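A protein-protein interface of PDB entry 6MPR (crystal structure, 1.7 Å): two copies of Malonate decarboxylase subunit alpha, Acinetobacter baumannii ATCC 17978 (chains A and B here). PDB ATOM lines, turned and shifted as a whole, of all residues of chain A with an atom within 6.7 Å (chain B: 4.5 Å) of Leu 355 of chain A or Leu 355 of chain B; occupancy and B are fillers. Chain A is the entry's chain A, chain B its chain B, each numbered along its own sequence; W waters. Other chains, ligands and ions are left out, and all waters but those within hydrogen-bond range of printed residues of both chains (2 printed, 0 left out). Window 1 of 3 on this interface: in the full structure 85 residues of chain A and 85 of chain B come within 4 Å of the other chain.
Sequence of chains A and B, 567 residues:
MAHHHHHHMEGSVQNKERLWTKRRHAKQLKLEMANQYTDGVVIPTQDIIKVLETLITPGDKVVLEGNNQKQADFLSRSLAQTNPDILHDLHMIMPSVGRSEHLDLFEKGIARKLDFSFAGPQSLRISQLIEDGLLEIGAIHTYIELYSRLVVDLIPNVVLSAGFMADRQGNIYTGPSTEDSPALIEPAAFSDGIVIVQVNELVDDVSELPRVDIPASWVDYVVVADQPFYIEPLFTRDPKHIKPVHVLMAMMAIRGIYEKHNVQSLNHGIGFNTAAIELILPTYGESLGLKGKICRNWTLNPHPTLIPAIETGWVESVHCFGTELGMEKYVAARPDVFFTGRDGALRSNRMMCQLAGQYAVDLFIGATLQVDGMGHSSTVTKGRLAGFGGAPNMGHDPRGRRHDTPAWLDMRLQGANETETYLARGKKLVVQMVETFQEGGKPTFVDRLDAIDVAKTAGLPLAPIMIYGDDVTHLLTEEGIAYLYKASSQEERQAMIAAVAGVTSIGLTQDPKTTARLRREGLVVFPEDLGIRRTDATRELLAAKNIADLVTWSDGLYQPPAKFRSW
Of the printed residues of chain B, Ile 144 of chain A touches Leu 355 and Tyr 359.
Printed residues of chain B within 4 Å of Glu 145 of chain A: Tyr 359 (3.5 Å).
Printed residues of chain B within 4 Å of Ser 148 of chain A: Leu 355, Ala 356, Tyr 359 and Ala 360.
Asn 349 of chain A touches none of the printed residues of chain B.
Printed residues of chain B within 4 Å of Leu 355 of chain A: Ser 148 (3.1 Å) and Leu 355 (3.7 Å).
Gly 357 of chain A touches none of the printed residues of chain B.
Printed residues of chain B within 4 Å of Tyr 359 of chain A: Ile 144 (3.6 Å), Ser 148 (3.98 Å) and Gln 358 (3.98 Å).
Printed residues of chain A within 4 Å of Leu 355 of chain B: Ile 144 (3.7 Å), Ser 148 (3.9 Å), Met 351 (3.5 Å) and Leu 355 (3.7 Å).
Of the printed residues of chain A, Tyr 359 of chain B touches Ile 144 (3.8 Å), Glu 145 (3.5 Å), Ser 148 (3.3 Å), Gln 358 (3.9 Å) and Asn 393 (2.8 Å).
The nearest printed residue of chain B that does not touch Leu 355 of chain A is Ile 144 of chain B (4.1 Å).
The nearest printed residue of chain B that does not touch Ile 144 of chain A is Gln 358 of chain B (5.9 Å).
O of Glu 145 of chain A lies within hydrogen-bond range of OG of Ser 148 of chain A, 2.7 Å away.
The side-chain amide oxygen of Asn 349 of chain A sits close to the backbone NH of Met 351 of chain A, 3.4 Å away.
The side-chain amide oxygen (OE1) of Gln 354 of chain A sits at hydrogen-bond distance from the side-chain amide nitrogen (ND2) of Asn 393 of chain A, at 2.9 Å.
N of Val 361 of chain A is in hydrogen-bond range of O of Ala 356 of chain A, at 3.3 Å.
The side-chain amide oxygen (OD1) of Asn 393 of chain A sits at hydrogen-bond distance from the side-chain amide nitrogen (NE2) of Gln 358 of chain A, 3.1 Å away.
OG of Ser 148 of chain B is in hydrogen-bond range of O of Ile 144 of chain B (2.7 Å).
Of the 21 printed residues of chain A, 10 touch a printed residue of chain B.
Hydrophobic or aromatic side chains of chain A within 4 Å of the printed part of chain B: Ile 144, Met 351, Leu 355, Ala 356, Tyr 359 and Ala 360.
Along chain A the printed residues that touch a printed residue of chain B span positions 144 to 393.
Printed residues of chain B that touch a printed residue of chain A: Ile 144, Ser 148, Met 351, Leu 355, Ala 356, Gln 358, Tyr 359 and Ala 360.
Hydrophobic or aromatic side chains of chain B within 4 Å of the printed part of chain A: Ile 144, Met 351, Leu 355, Ala 356, Tyr 359 and Ala 360.
Among the printed residues, no Asp or Glu carboxylate lies within 4 Å of a Lys or Arg side-chain nitrogen of the other chain.
Among the printed residues, pairs that only touch across the chains: Ile 144 of chain A with Leu 355 of chain B, Ile 144 of chain A with Tyr 359 of chain B, Glu 145 of chain A with Tyr 359 of chain B, Ser 148 of chain A with Leu 355 of chain B, Ser 148 of chain A with Ala 356 of chain B, Ser 148 of chain A with Tyr 359 of chain B, Ser 148 of chain A with Ala 360 of chain B, Met 351 of chain A with Met 351 of chain B, Met 351 of chain A with Leu 355 of chain B, Leu 355 of chain A with Ser 148 of chain B, Leu 355 of chain A with Leu 355 of chain B, Ala 356 of chain A with Ser 148 of chain B, Gln 358 of chain A with Tyr 359 of chain B, Tyr 359 of chain A with Ile 144 of chain B, Tyr 359 of chain A with Ser 148 of chain B, Tyr 359 of chain A with Gln 358 of chain B and Ala 360 of chain A with Ser 148 of chain B.
Water W2 bridges O of Met 352 of chain A (3.0 Å) and OG of Ser 148 of chain B (3.2 Å).
Water W1 bridges the side-chain amide oxygen (OE1) of Gln 358 of chain A (3.1 Å) and the side-chain amide nitrogen (NE2) of Gln 358 of chain B (3.2 Å).
NE2 of Gln 358 of chain B sits at hydrogen-bond distance from OE1 of Gln 358 of chain A (3.1 Å).
The side-chain hydroxyl of Tyr 359 of chain B sits at hydrogen-bond distance from the side-chain amide oxygen of Asn 393 of chain A, 2.8 Å away.
Ile 144 of chain A touches Tyr 359 of chain B, and with the chains exchanged Tyr 359 of chain A touches Ile 144 of chain B.
Ser 148 of chain A touches Ala 356 of chain B, and with the chains exchanged Ala 356 of chain A touches Ser 148 of chain B.
Ser 148 of chain A touches Ala 360 of chain B, and with the chains exchanged Ala 360 of chain A touches Ser 148 of chain B.
Met 351 of chain B touches its own counterpart, Met 351 of chain A.
Positions printed for both chains: 144, 148, 351, 352, 353, 354, 355, 356, 357, 358, 359 and 360.
Of the 19 pairs that touch across the chains among the printed residues, 15 have their exchanged pair printed and touching as well.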
ATOM      1  N   ILE A 144      19.879  18.263  29.864  1.00  0.00           N
ATOM      2  CA  ILE A 144      19.115  19.454  29.508  1.00  0.00           C
ATOM      3  C   ILE A 144      18.099  19.821  30.577  1.00  0.00           C
ATOM      4  O   ILE A 144      17.648  20.967  30.609  1.00  0.00           O
ATOM      5  CB  ILE A 144      18.417  19.332  28.140  1.00  0.00           C
ATOM      6  CG1 ILE A 144      17.404  18.189  28.134  1.00  0.00           C
ATOM      7  CG2 ILE A 144      19.469  19.201  27.033  1.00  0.00           C
ATOM      8  CD1 ILE A 144      16.584  18.143  26.864  1.00  0.00           C
ATOM      9  N   GLU A 145      17.737  18.885  31.463  1.00  0.00           N
ATOM     10  CA  GLU A 145      16.989  19.253  32.667  1.00  0.00           C
ATOM     11  C   GLU A 145      17.804  20.187  33.555  1.00  0.00           C
ATOM     12  O   GLU A 145      17.291  21.198  34.059  1.00  0.00           O
ATOM     13  CB  GLU A 145      16.586  17.979  33.424  1.00  0.00           C
ATOM     14  CG  GLU A 145      15.862  18.178  34.747  1.00  0.00           C
ATOM     15  CD  GLU A 145      15.739  16.860  35.518  1.00  0.00           C
ATOM     16  OE1 GLU A 145      14.973  16.809  36.505  1.00  0.00           O
ATOM     17  OE2 GLU A 145      16.444  15.886  35.155  1.00  0.00           O
ATOM     18  N   TYR A 147      20.309  22.142  32.568  1.00  0.00           N
ATOM     19  CA  TYR A 147      20.410  23.447  31.903  1.00  0.00           C
ATOM     20  C   TYR A 147      19.147  24.270  32.121  1.00  0.00           C
ATOM     21  O   TYR A 147      19.206  25.501  32.247  1.00  0.00           O
ATOM     22  CB  TYR A 147      20.623  23.323  30.388  1.00  0.00           C
ATOM     23  CG  TYR A 147      21.722  22.413  29.900  1.00  0.00           C
ATOM     24  CD1 TYR A 147      22.828  22.129  30.682  1.00  0.00           C
ATOM     25  CD2 TYR A 147      21.646  21.843  28.615  1.00  0.00           C
ATOM     26  CE1 TYR A 147      23.815  21.275  30.230  1.00  0.00           C
ATOM     27  CE2 TYR A 147      22.625  20.987  28.156  1.00  0.00           C
ATOM     28  CZ  TYR A 147      23.708  20.709  28.965  1.00  0.00           C
ATOM     29  OH  TYR A 147      24.702  19.872  28.527  1.00  0.00           O
ATOM     30  N   SER A 148      17.989  23.611  32.104  1.00  0.00           N
ATOM     31  CA  SER A 148      16.725  24.335  32.178  1.00  0.00           C
ATOM     32  C   SER A 148      16.532  25.007  33.529  1.00  0.00           C
ATOM     33  O   SER A 148      15.869  26.042  33.602  1.00  0.00           O
ATOM     34  CB  SER A 148      15.560  23.391  31.887  1.00  0.00           C
ATOM     35  OG  SER A 148      15.248  22.613  33.031  1.00  0.00           O
ATOM     36  N   THR A 299      21.515  11.664  15.921  1.00  0.00           N
ATOM     37  CA  THR A 299      22.008  12.533  16.980  1.00  0.00           C
ATOM     38  C   THR A 299      23.089  11.732  17.689  1.00  0.00           C
ATOM     39  O   THR A 299      22.790  10.743  18.377  1.00  0.00           O
ATOM     40  CB  THR A 299      20.900  12.959  17.944  1.00  0.00           C
ATOM     41  OG1 THR A 299      20.268  11.790  18.488  1.00  0.00           O
ATOM     42  CG2 THR A 299      19.865  13.800  17.226  1.00  0.00           C
ATOM     43  N   PHE A 321      26.598  16.154  19.999  1.00  0.00           N
ATOM     44  CA  PHE A 321      26.663  16.741  21.333  1.00  0.00           C
ATOM     45  C   PHE A 321      28.020  17.380  21.606  1.00  0.00           C
ATOM     46  O   PHE A 321      28.107  18.350  22.368  1.00  0.00           O
ATOM     47  CB  PHE A 321      26.413  15.673  22.399  1.00  0.00           C
ATOM     48  CG  PHE A 321      25.264  14.752  22.113  1.00  0.00           C
ATOM     49  CD1 PHE A 321      23.972  15.100  22.471  1.00  0.00           C
ATOM     50  CD2 PHE A 321      25.485  13.529  21.507  1.00  0.00           C
ATOM     51  CE1 PHE A 321      22.915  14.234  22.238  1.00  0.00           C
ATOM     52  CE2 PHE A 321      24.436  12.653  21.263  1.00  0.00           C
ATOM     53  CZ  PHE A 321      23.148  13.005  21.614  1.00  0.00           C
ATOM     54  N   ASN A 349      26.562  21.042  19.826  1.00  0.00           N
ATOM     55  CA  ASN A 349      25.655  21.816  20.655  1.00  0.00           C
ATOM     56  C   ASN A 349      24.889  20.788  21.486  1.00  0.00           C
ATOM     57  O   ASN A 349      23.930  20.201  20.990  1.00  0.00           O
ATOM     58  CB  ASN A 349      24.734  22.666  19.786  1.00  0.00           C
ATOM     59  CG  ASN A 349      23.821  23.571  20.586  1.00  0.00           C
ATOM     60  OD1 ASN A 349      23.394  23.230  21.692  1.00  0.00           O
ATOM     61  ND2 ASN A 349      23.495  24.737  20.014  1.00  0.00           N
ATOM     62  N   ARG A 350      25.331  20.566  22.730  1.00  0.00           N
ATOM     63  CA  ARG A 350      24.752  19.461  23.500  1.00  0.00           C
ATOM     64  C   ARG A 350      23.281  19.712  23.809  1.00  0.00           C
ATOM     65  O   ARG A 350      22.461  18.784  23.737  1.00  0.00           O
ATOM     66  CB  ARG A 350      25.554  19.200  24.787  1.00  0.00           C
ATOM     67  CG  ARG A 350      24.899  18.127  25.700  1.00  0.00           C
ATOM     68  CD  ARG A 350      25.889  17.501  26.690  1.00  0.00           C
ATOM     69  NE  ARG A 350      26.733  16.502  26.032  1.00  0.00           N
ATOM     70  CZ  ARG A 350      28.035  16.636  25.798  1.00  0.00           C
ATOM     71  NH1 ARG A 350      28.678  17.721  26.195  1.00  0.00           N
ATOM     72  NH2 ARG A 350      28.710  15.674  25.173  1.00  0.00           N
ATOM     73  N   MET A 351      22.909  20.955  24.124  1.00  0.00           N
ATOM     74  CA  MET A 351      21.498  21.238  24.387  1.00  0.00           C
ATOM     75  C   MET A 351      20.638  20.943  23.162  1.00  0.00           C
ATOM     76  O   MET A 351      19.589  20.285  23.265  1.00  0.00           O
ATOM     77  CB  MET A 351      21.301  22.687  24.831  1.00  0.00           C
ATOM     78  CG  MET A 351      19.815  23.030  24.957  1.00  0.00           C
ATOM     79  SD  MET A 351      19.385  24.145  26.288  1.00  0.00           S
ATOM     80  CE  MET A 351      19.607  25.745  25.540  1.00  0.00           C
ATOM     81  N   MET A 352      21.062  21.417  21.986  1.00  0.00           N
ATOM     82  CA  MET A 352      20.253  21.216  20.783  1.00  0.00           C
ATOM     83  C   MET A 352      20.193  19.748  20.391  1.00  0.00           C
ATOM     84  O   MET A 352      19.135  19.242  19.979  1.00  0.00           O
ATOM     85  CB  MET A 352      20.803  22.076  19.644  1.00  0.00           C
ATOM     86  CG  MET A 352      20.043  21.997  18.322  1.00  0.00           C
ATOM     87  SD  MET A 352      20.831  23.124  17.138  1.00  0.00           S
ATOM     88  CE  MET A 352      20.254  24.700  17.771  1.00  0.00           C
ATOM     89  N   CYS A 353      21.314  19.046  20.540  1.00  0.00           N
ATOM     90  CA  CYS A 353      21.363  17.645  20.162  1.00  0.00           C
ATOM     91  C   CYS A 353      20.538  16.791  21.119  1.00  0.00           C
ATOM     92  O   CYS A 353      19.820  15.889  20.686  1.00  0.00           O
ATOM     93  CB  CYS A 353      22.818  17.187  20.135  1.00  0.00           C
ATOM     94  SG  CYS A 353      23.109  15.712  19.187  1.00  0.00           S
ATOM     95  N   GLN A 354      20.638  17.054  22.428  1.00  0.00           N
ATOM     96  CA  GLN A 354      19.795  16.336  23.390  1.00  0.00           C
ATOM     97  C   GLN A 354      18.316  16.619  23.155  1.00  0.00           C
ATOM     98  O   GLN A 354      17.482  15.711  23.249  1.00  0.00           O
ATOM     99  CB  GLN A 354      20.181  16.722  24.813  1.00  0.00           C
ATOM    100  CG  GLN A 354      21.432  16.040  25.336  1.00  0.00           C
ATOM    101  CD  GLN A 354      21.186  14.599  25.712  1.00  0.00           C
ATOM    102  OE1 GLN A 354      20.105  14.252  26.190  1.00  0.00           O
ATOM    103  NE2 GLN A 354      22.182  13.748  25.498  1.00  0.00           N
ATOM    104  N   LEU A 355      17.968  17.877  22.847  1.00  0.00           N
ATOM    105  CA  LEU A 355      16.575  18.190  22.522  1.00  0.00           C
ATOM    106  C   LEU A 355      16.091  17.377  21.322  1.00  0.00           C
ATOM    107  O   LEU A 355      14.989  16.809  21.345  1.00  0.00           O
ATOM    108  CB  LEU A 355      16.424  19.685  22.245  1.00  0.00           C
ATOM    109  CG  LEU A 355      14.987  20.201  22.302  1.00  0.00           C
ATOM    110  CD1 LEU A 355      14.352  19.901  23.669  1.00  0.00           C
ATOM    111  CD2 LEU A 355      14.966  21.693  21.998  1.00  0.00           C
ATOM    112  N   ALA A 356      16.891  17.325  20.254  1.00  0.00           N
ATOM    113  CA  ALA A 356      16.514  16.498  19.110  1.00  0.00           C
ATOM    114  C   ALA A 356      16.435  15.032  19.498  1.00  0.00           C
ATOM    115  O   ALA A 356      15.564  14.301  19.012  1.00  0.00           O
ATOM    116  CB  ALA A 356      17.500  16.687  17.957  1.00  0.00           C
ATOM    117  N   GLY A 357      17.340  14.582  20.368  1.00  0.00           N
ATOM    118  CA  GLY A 357      17.284  13.201  20.815  1.00  0.00           C
ATOM    119  C   GLY A 357      15.983  12.867  21.517  1.00  0.00           C
ATOM    120  O   GLY A 357      15.529  11.722  21.482  1.00  0.00           O
ATOM    121  N   GLN A 358      15.380  13.849  22.184  1.00  0.00           N
ATOM    122  CA  GLN A 358      14.079  13.628  22.811  1.00  0.00           C
ATOM    123  C   GLN A 358      12.940  13.704  21.793  1.00  0.00           C
ATOM    124  O   GLN A 358      12.104  12.799  21.707  1.00  0.00           O
ATOM    125  CB  GLN A 358      13.836  14.663  23.916  1.00  0.00           C
ATOM    126  CG  GLN A 358      12.376  14.581  24.390  1.00  0.00           C
ATOM    127  CD  GLN A 358      11.963  15.681  25.349  1.00  0.00           C
ATOM    128  OE1 GLN A 358      10.783  15.799  25.668  1.00  0.00           O
ATOM    129  NE2 GLN A 358      12.919  16.472  25.821  1.00  0.00           N
ATOM    130  N   TYR A 359      12.880  14.791  21.029  1.00  0.00           N
ATOM    131  CA  TYR A 359      11.678  15.138  20.283  1.00  0.00           C
ATOM    132  C   TYR A 359      11.702  14.734  18.819  1.00  0.00           C
ATOM    133  O   TYR A 359      10.633  14.661  18.206  1.00  0.00           O
ATOM    134  CB  TYR A 359      11.442  16.653  20.338  1.00  0.00           C
ATOM    135  CG  TYR A 359      10.504  17.118  21.409  1.00  0.00           C
ATOM    136  CD1 TYR A 359       9.180  16.710  21.425  1.00  0.00           C
ATOM    137  CD2 TYR A 359      10.923  17.999  22.382  1.00  0.00           C
ATOM    138  CE1 TYR A 359       8.308  17.158  22.401  1.00  0.00           C
ATOM    139  CE2 TYR A 359      10.059  18.455  23.351  1.00  0.00           C
ATOM    140  CZ  TYR A 359       8.752  18.030  23.350  1.00  0.00           C
ATOM    141  OH  TYR A 359       7.892  18.486  24.310  1.00  0.00           O
ATOM    142  N   ALA A 360      12.875  14.517  18.226  1.00  0.00           N
ATOM    143  CA  ALA A 360      12.977  14.412  16.777  1.00  0.00           C
ATOM    144  C   ALA A 360      13.453  13.067  16.246  1.00  0.00           C
ATOM    145  O   ALA A 360      13.367  12.853  15.032  1.00  0.00           O
ATOM    146  CB  ALA A 360      13.909  15.506  16.229  1.00  0.00           C
ATOM    147  N   VAL A 361      13.940  12.150  17.081  1.00  0.00           N
ATOM    148  CA  VAL A 361      14.426  10.876  16.560  1.00  0.00           C
ATOM    149  C   VAL A 361      13.480   9.740  16.951  1.00  0.00           C
ATOM    150  O   VAL A 361      12.753   9.800  17.953  1.00  0.00           O
ATOM    151  CB  VAL A 361      15.872  10.540  16.985  1.00  0.00           C
ATOM    152  CG1 VAL A 361      16.836  11.671  16.595  1.00  0.00           C
ATOM    153  CG2 VAL A 361      15.959  10.196  18.455  1.00  0.00           C
ATOM    154  N   ASN A 393      16.847  11.598  29.424  1.00  0.00           N
ATOM    155  CA  ASN A 393      16.227  12.396  28.373  1.00  0.00           C
ATOM    156  C   ASN A 393      16.095  11.602  27.081  1.00  0.00           C
ATOM    157  O   ASN A 393      15.114  11.753  26.349  1.00  0.00           O
ATOM    158  CB  ASN A 393      17.041  13.665  28.139  1.00  0.00           C
ATOM    159  CG  ASN A 393      16.490  14.502  26.998  1.00  0.00           C
ATOM    160  OD1 ASN A 393      15.383  15.036  27.090  1.00  0.00           O
ATOM    161  ND2 ASN A 393      17.253  14.601  25.907  1.00  0.00           N
ATOM    162  N   MET A 394      17.071  10.745  26.798  1.00  0.00           N
ATOM    163  CA  MET A 394      16.999   9.919  25.602  1.00  0.00           C
ATOM    164  C   MET A 394      16.082   8.715  25.791  1.00  0.00           C
ATOM    165  O   MET A 394      15.417   8.295  24.830  1.00  0.00           O
ATOM    166  CB  MET A 394      18.406   9.467  25.217  1.00  0.00           C
ATOM    167  CG  MET A 394      19.413  10.605  25.160  1.00  0.00           C
ATOM    168  SD  MET A 394      19.017  11.791  23.851  1.00  0.00           S
ATOM    169  CE  MET A 394      19.183  10.713  22.455  1.00  0.00           C
ATOM    170  N   ILE B 144       9.115  23.586  20.425  1.00  0.00           N
ATOM    171  CA  ILE B 144      10.502  23.125  20.501  1.00  0.00           C
ATOM    172  C   ILE B 144      10.679  21.795  19.812  1.00  0.00           C
ATOM    173  O   ILE B 144      11.808  21.441  19.451  1.00  0.00           O
ATOM    174  CB  ILE B 144      11.032  23.022  21.935  1.00  0.00           C
ATOM    175  CG1 ILE B 144      10.220  22.031  22.764  1.00  0.00           C
ATOM    176  CG2 ILE B 144      11.051  24.410  22.544  1.00  0.00           C
ATOM    177  CD1 ILE B 144      10.724  21.965  24.195  1.00  0.00           C
ATOM    178  N   SER B 148      13.546  21.077  17.052  1.00  0.00           N
ATOM    179  CA  SER B 148      14.428  19.923  17.179  1.00  0.00           C
ATOM    180  C   SER B 148      14.574  19.181  15.859  1.00  0.00           C
ATOM    181  O   SER B 148      15.639  18.615  15.586  1.00  0.00           O
ATOM    182  CB  SER B 148      13.907  18.990  18.269  1.00  0.00           C
ATOM    183  OG  SER B 148      13.875  19.686  19.500  1.00  0.00           O
ATOM    184  N   MET B 351      13.182  28.860  22.780  1.00  0.00           N
ATOM    185  CA  MET B 351      13.626  27.483  22.974  1.00  0.00           C
ATOM    186  C   MET B 351      14.014  27.240  24.430  1.00  0.00           C
ATOM    187  O   MET B 351      13.560  26.269  25.056  1.00  0.00           O
ATOM    188  CB  MET B 351      14.789  27.174  22.026  1.00  0.00           C
ATOM    189  CG  MET B 351      15.351  25.750  22.143  1.00  0.00           C
ATOM    190  SD  MET B 351      16.447  25.593  23.556  1.00  0.00           S
ATOM    191  CE  MET B 351      17.540  26.997  23.331  1.00  0.00           C
ATOM    192  N   MET B 352      14.845  28.124  24.993  1.00  0.00           N
ATOM    193  CA  MET B 352      15.295  27.963  26.372  1.00  0.00           C
ATOM    194  C   MET B 352      14.125  28.043  27.342  1.00  0.00           C
ATOM    195  O   MET B 352      14.043  27.261  28.297  1.00  0.00           O
ATOM    196  CB  MET B 352      16.340  29.033  26.704  1.00  0.00           C
ATOM    197  CG  MET B 352      16.956  28.943  28.076  1.00  0.00           C
ATOM    198  SD  MET B 352      18.241  30.220  28.230  1.00  0.00           S
ATOM    199  CE  MET B 352      19.583  29.505  27.273  1.00  0.00           C
ATOM    200  N   CYS B 353      13.207  28.983  27.109  1.00  0.00           N
ATOM    201  CA  CYS B 353      12.070  29.148  28.012  1.00  0.00           C
ATOM    202  C   CYS B 353      11.120  27.951  27.939  1.00  0.00           C
ATOM    203  O   CYS B 353      10.614  27.486  28.966  1.00  0.00           O
ATOM    204  CB  CYS B 353      11.340  30.446  27.668  1.00  0.00           C
ATOM    205  SG  CYS B 353      10.294  31.065  28.991  1.00  0.00           S
ATOM    206  N   GLN B 354      10.839  27.454  26.729  1.00  0.00           N
ATOM    207  CA  GLN B 354      10.005  26.263  26.620  1.00  0.00           C
ATOM    208  C   GLN B 354      10.660  25.055  27.271  1.00  0.00           C
ATOM    209  O   GLN B 354       9.967  24.193  27.823  1.00  0.00           O
ATOM    210  CB  GLN B 354       9.714  25.967  25.153  1.00  0.00           C
ATOM    211  CG  GLN B 354       8.700  26.889  24.527  1.00  0.00           C
ATOM    212  CD  GLN B 354       7.279  26.514  24.891  1.00  0.00           C
ATOM    213  OE1 GLN B 354       6.973  25.349  25.143  1.00  0.00           O
ATOM    214  NE2 GLN B 354       6.403  27.507  24.930  1.00  0.00           N
ATOM    215  N   LEU B 355      11.989  24.963  27.200  1.00  0.00           N
ATOM    216  CA  LEU B 355      12.678  23.836  27.822  1.00  0.00           C
ATOM    217  C   LEU B 355      12.541  23.883  29.332  1.00  0.00           C
ATOM    218  O   LEU B 355      12.258  22.862  29.969  1.00  0.00           O
ATOM    219  CB  LEU B 355      14.150  23.837  27.430  1.00  0.00           C
ATOM    220  CG  LEU B 355      14.919  22.582  27.832  1.00  0.00           C
ATOM    221  CD1 LEU B 355      14.426  21.338  27.097  1.00  0.00           C
ATOM    222  CD2 LEU B 355      16.415  22.795  27.632  1.00  0.00           C
ATOM    223  N   ALA B 356      12.723  25.067  29.923  1.00  0.00           N
ATOM    224  CA  ALA B 356      12.469  25.222  31.346  1.00  0.00           C
ATOM    225  C   ALA B 356      10.995  24.970  31.675  1.00  0.00           C
ATOM    226  O   ALA B 356      10.679  24.370  32.705  1.00  0.00           O
ATOM    227  CB  ALA B 356      12.895  26.620  31.795  1.00  0.00           C
ATOM    228  N   GLY B 357      10.088  25.411  30.804  1.00  0.00           N
ATOM    229  CA  GLY B 357       8.677  25.086  30.979  1.00  0.00           C
ATOM    230  C   GLY B 357       8.409  23.594  31.067  1.00  0.00           C
ATOM    231  O   GLY B 357       7.515  23.162  31.801  1.00  0.00           O
ATOM    232  N   GLN B 358       9.193  22.782  30.346  1.00  0.00           N
ATOM    233  CA  GLN B 358       9.039  21.329  30.421  1.00  0.00           C
ATOM    234  C   GLN B 358       9.719  20.730  31.655  1.00  0.00           C
ATOM    235  O   GLN B 358       9.106  19.958  32.398  1.00  0.00           O
ATOM    236  CB  GLN B 358       9.598  20.658  29.161  1.00  0.00           C
ATOM    237  CG  GLN B 358       9.671  19.142  29.366  1.00  0.00           C
ATOM    238  CD  GLN B 358      10.399  18.399  28.253  1.00  0.00           C
ATOM    239  OE1 GLN B 358      10.748  18.967  27.233  1.00  0.00           O
ATOM    240  NE2 GLN B 358      10.641  17.122  28.470  1.00  0.00           N
ATOM    241  N   TYR B 359      10.985  21.071  31.889  1.00  0.00           N
ATOM    242  CA  TYR B 359      11.826  20.330  32.816  1.00  0.00           C
ATOM    243  C   TYR B 359      12.018  20.986  34.170  1.00  0.00           C
ATOM    244  O   TYR B 359      12.426  20.294  35.108  1.00  0.00           O
ATOM    245  CB  TYR B 359      13.224  20.131  32.216  1.00  0.00           C
ATOM    246  CG  TYR B 359      13.425  18.827  31.480  1.00  0.00           C
ATOM    247  CD1 TYR B 359      13.376  17.615  32.150  1.00  0.00           C
ATOM    248  CD2 TYR B 359      13.684  18.817  30.125  1.00  0.00           C
ATOM    249  CE1 TYR B 359      13.571  16.422  31.490  1.00  0.00           C
ATOM    250  CE2 TYR B 359      13.899  17.610  29.434  1.00  0.00           C
ATOM    251  CZ  TYR B 359      13.831  16.421  30.134  1.00  0.00           C
ATOM    252  OH  TYR B 359      14.034  15.222  29.499  1.00  0.00           O
ATOM    253  N   ALA B 360      11.800  22.295  34.286  1.00  0.00           N
ATOM    254  CA  ALA B 360      12.231  23.026  35.470  1.00  0.00           C
ATOM    255  C   ALA B 360      11.121  23.627  36.322  1.00  0.00           C
ATOM    256  O   ALA B 360      11.407  24.054  37.449  1.00  0.00           O
ATOM    257  CB  ALA B 360      13.202  24.149  35.069  1.00  0.00           C
HETATM  258  O   HOH W   1       9.036  14.489  27.804  1.00  0.00           O
HETATM  259  O   HOH W   2      16.788  20.874  19.192  1.00  0.00           O
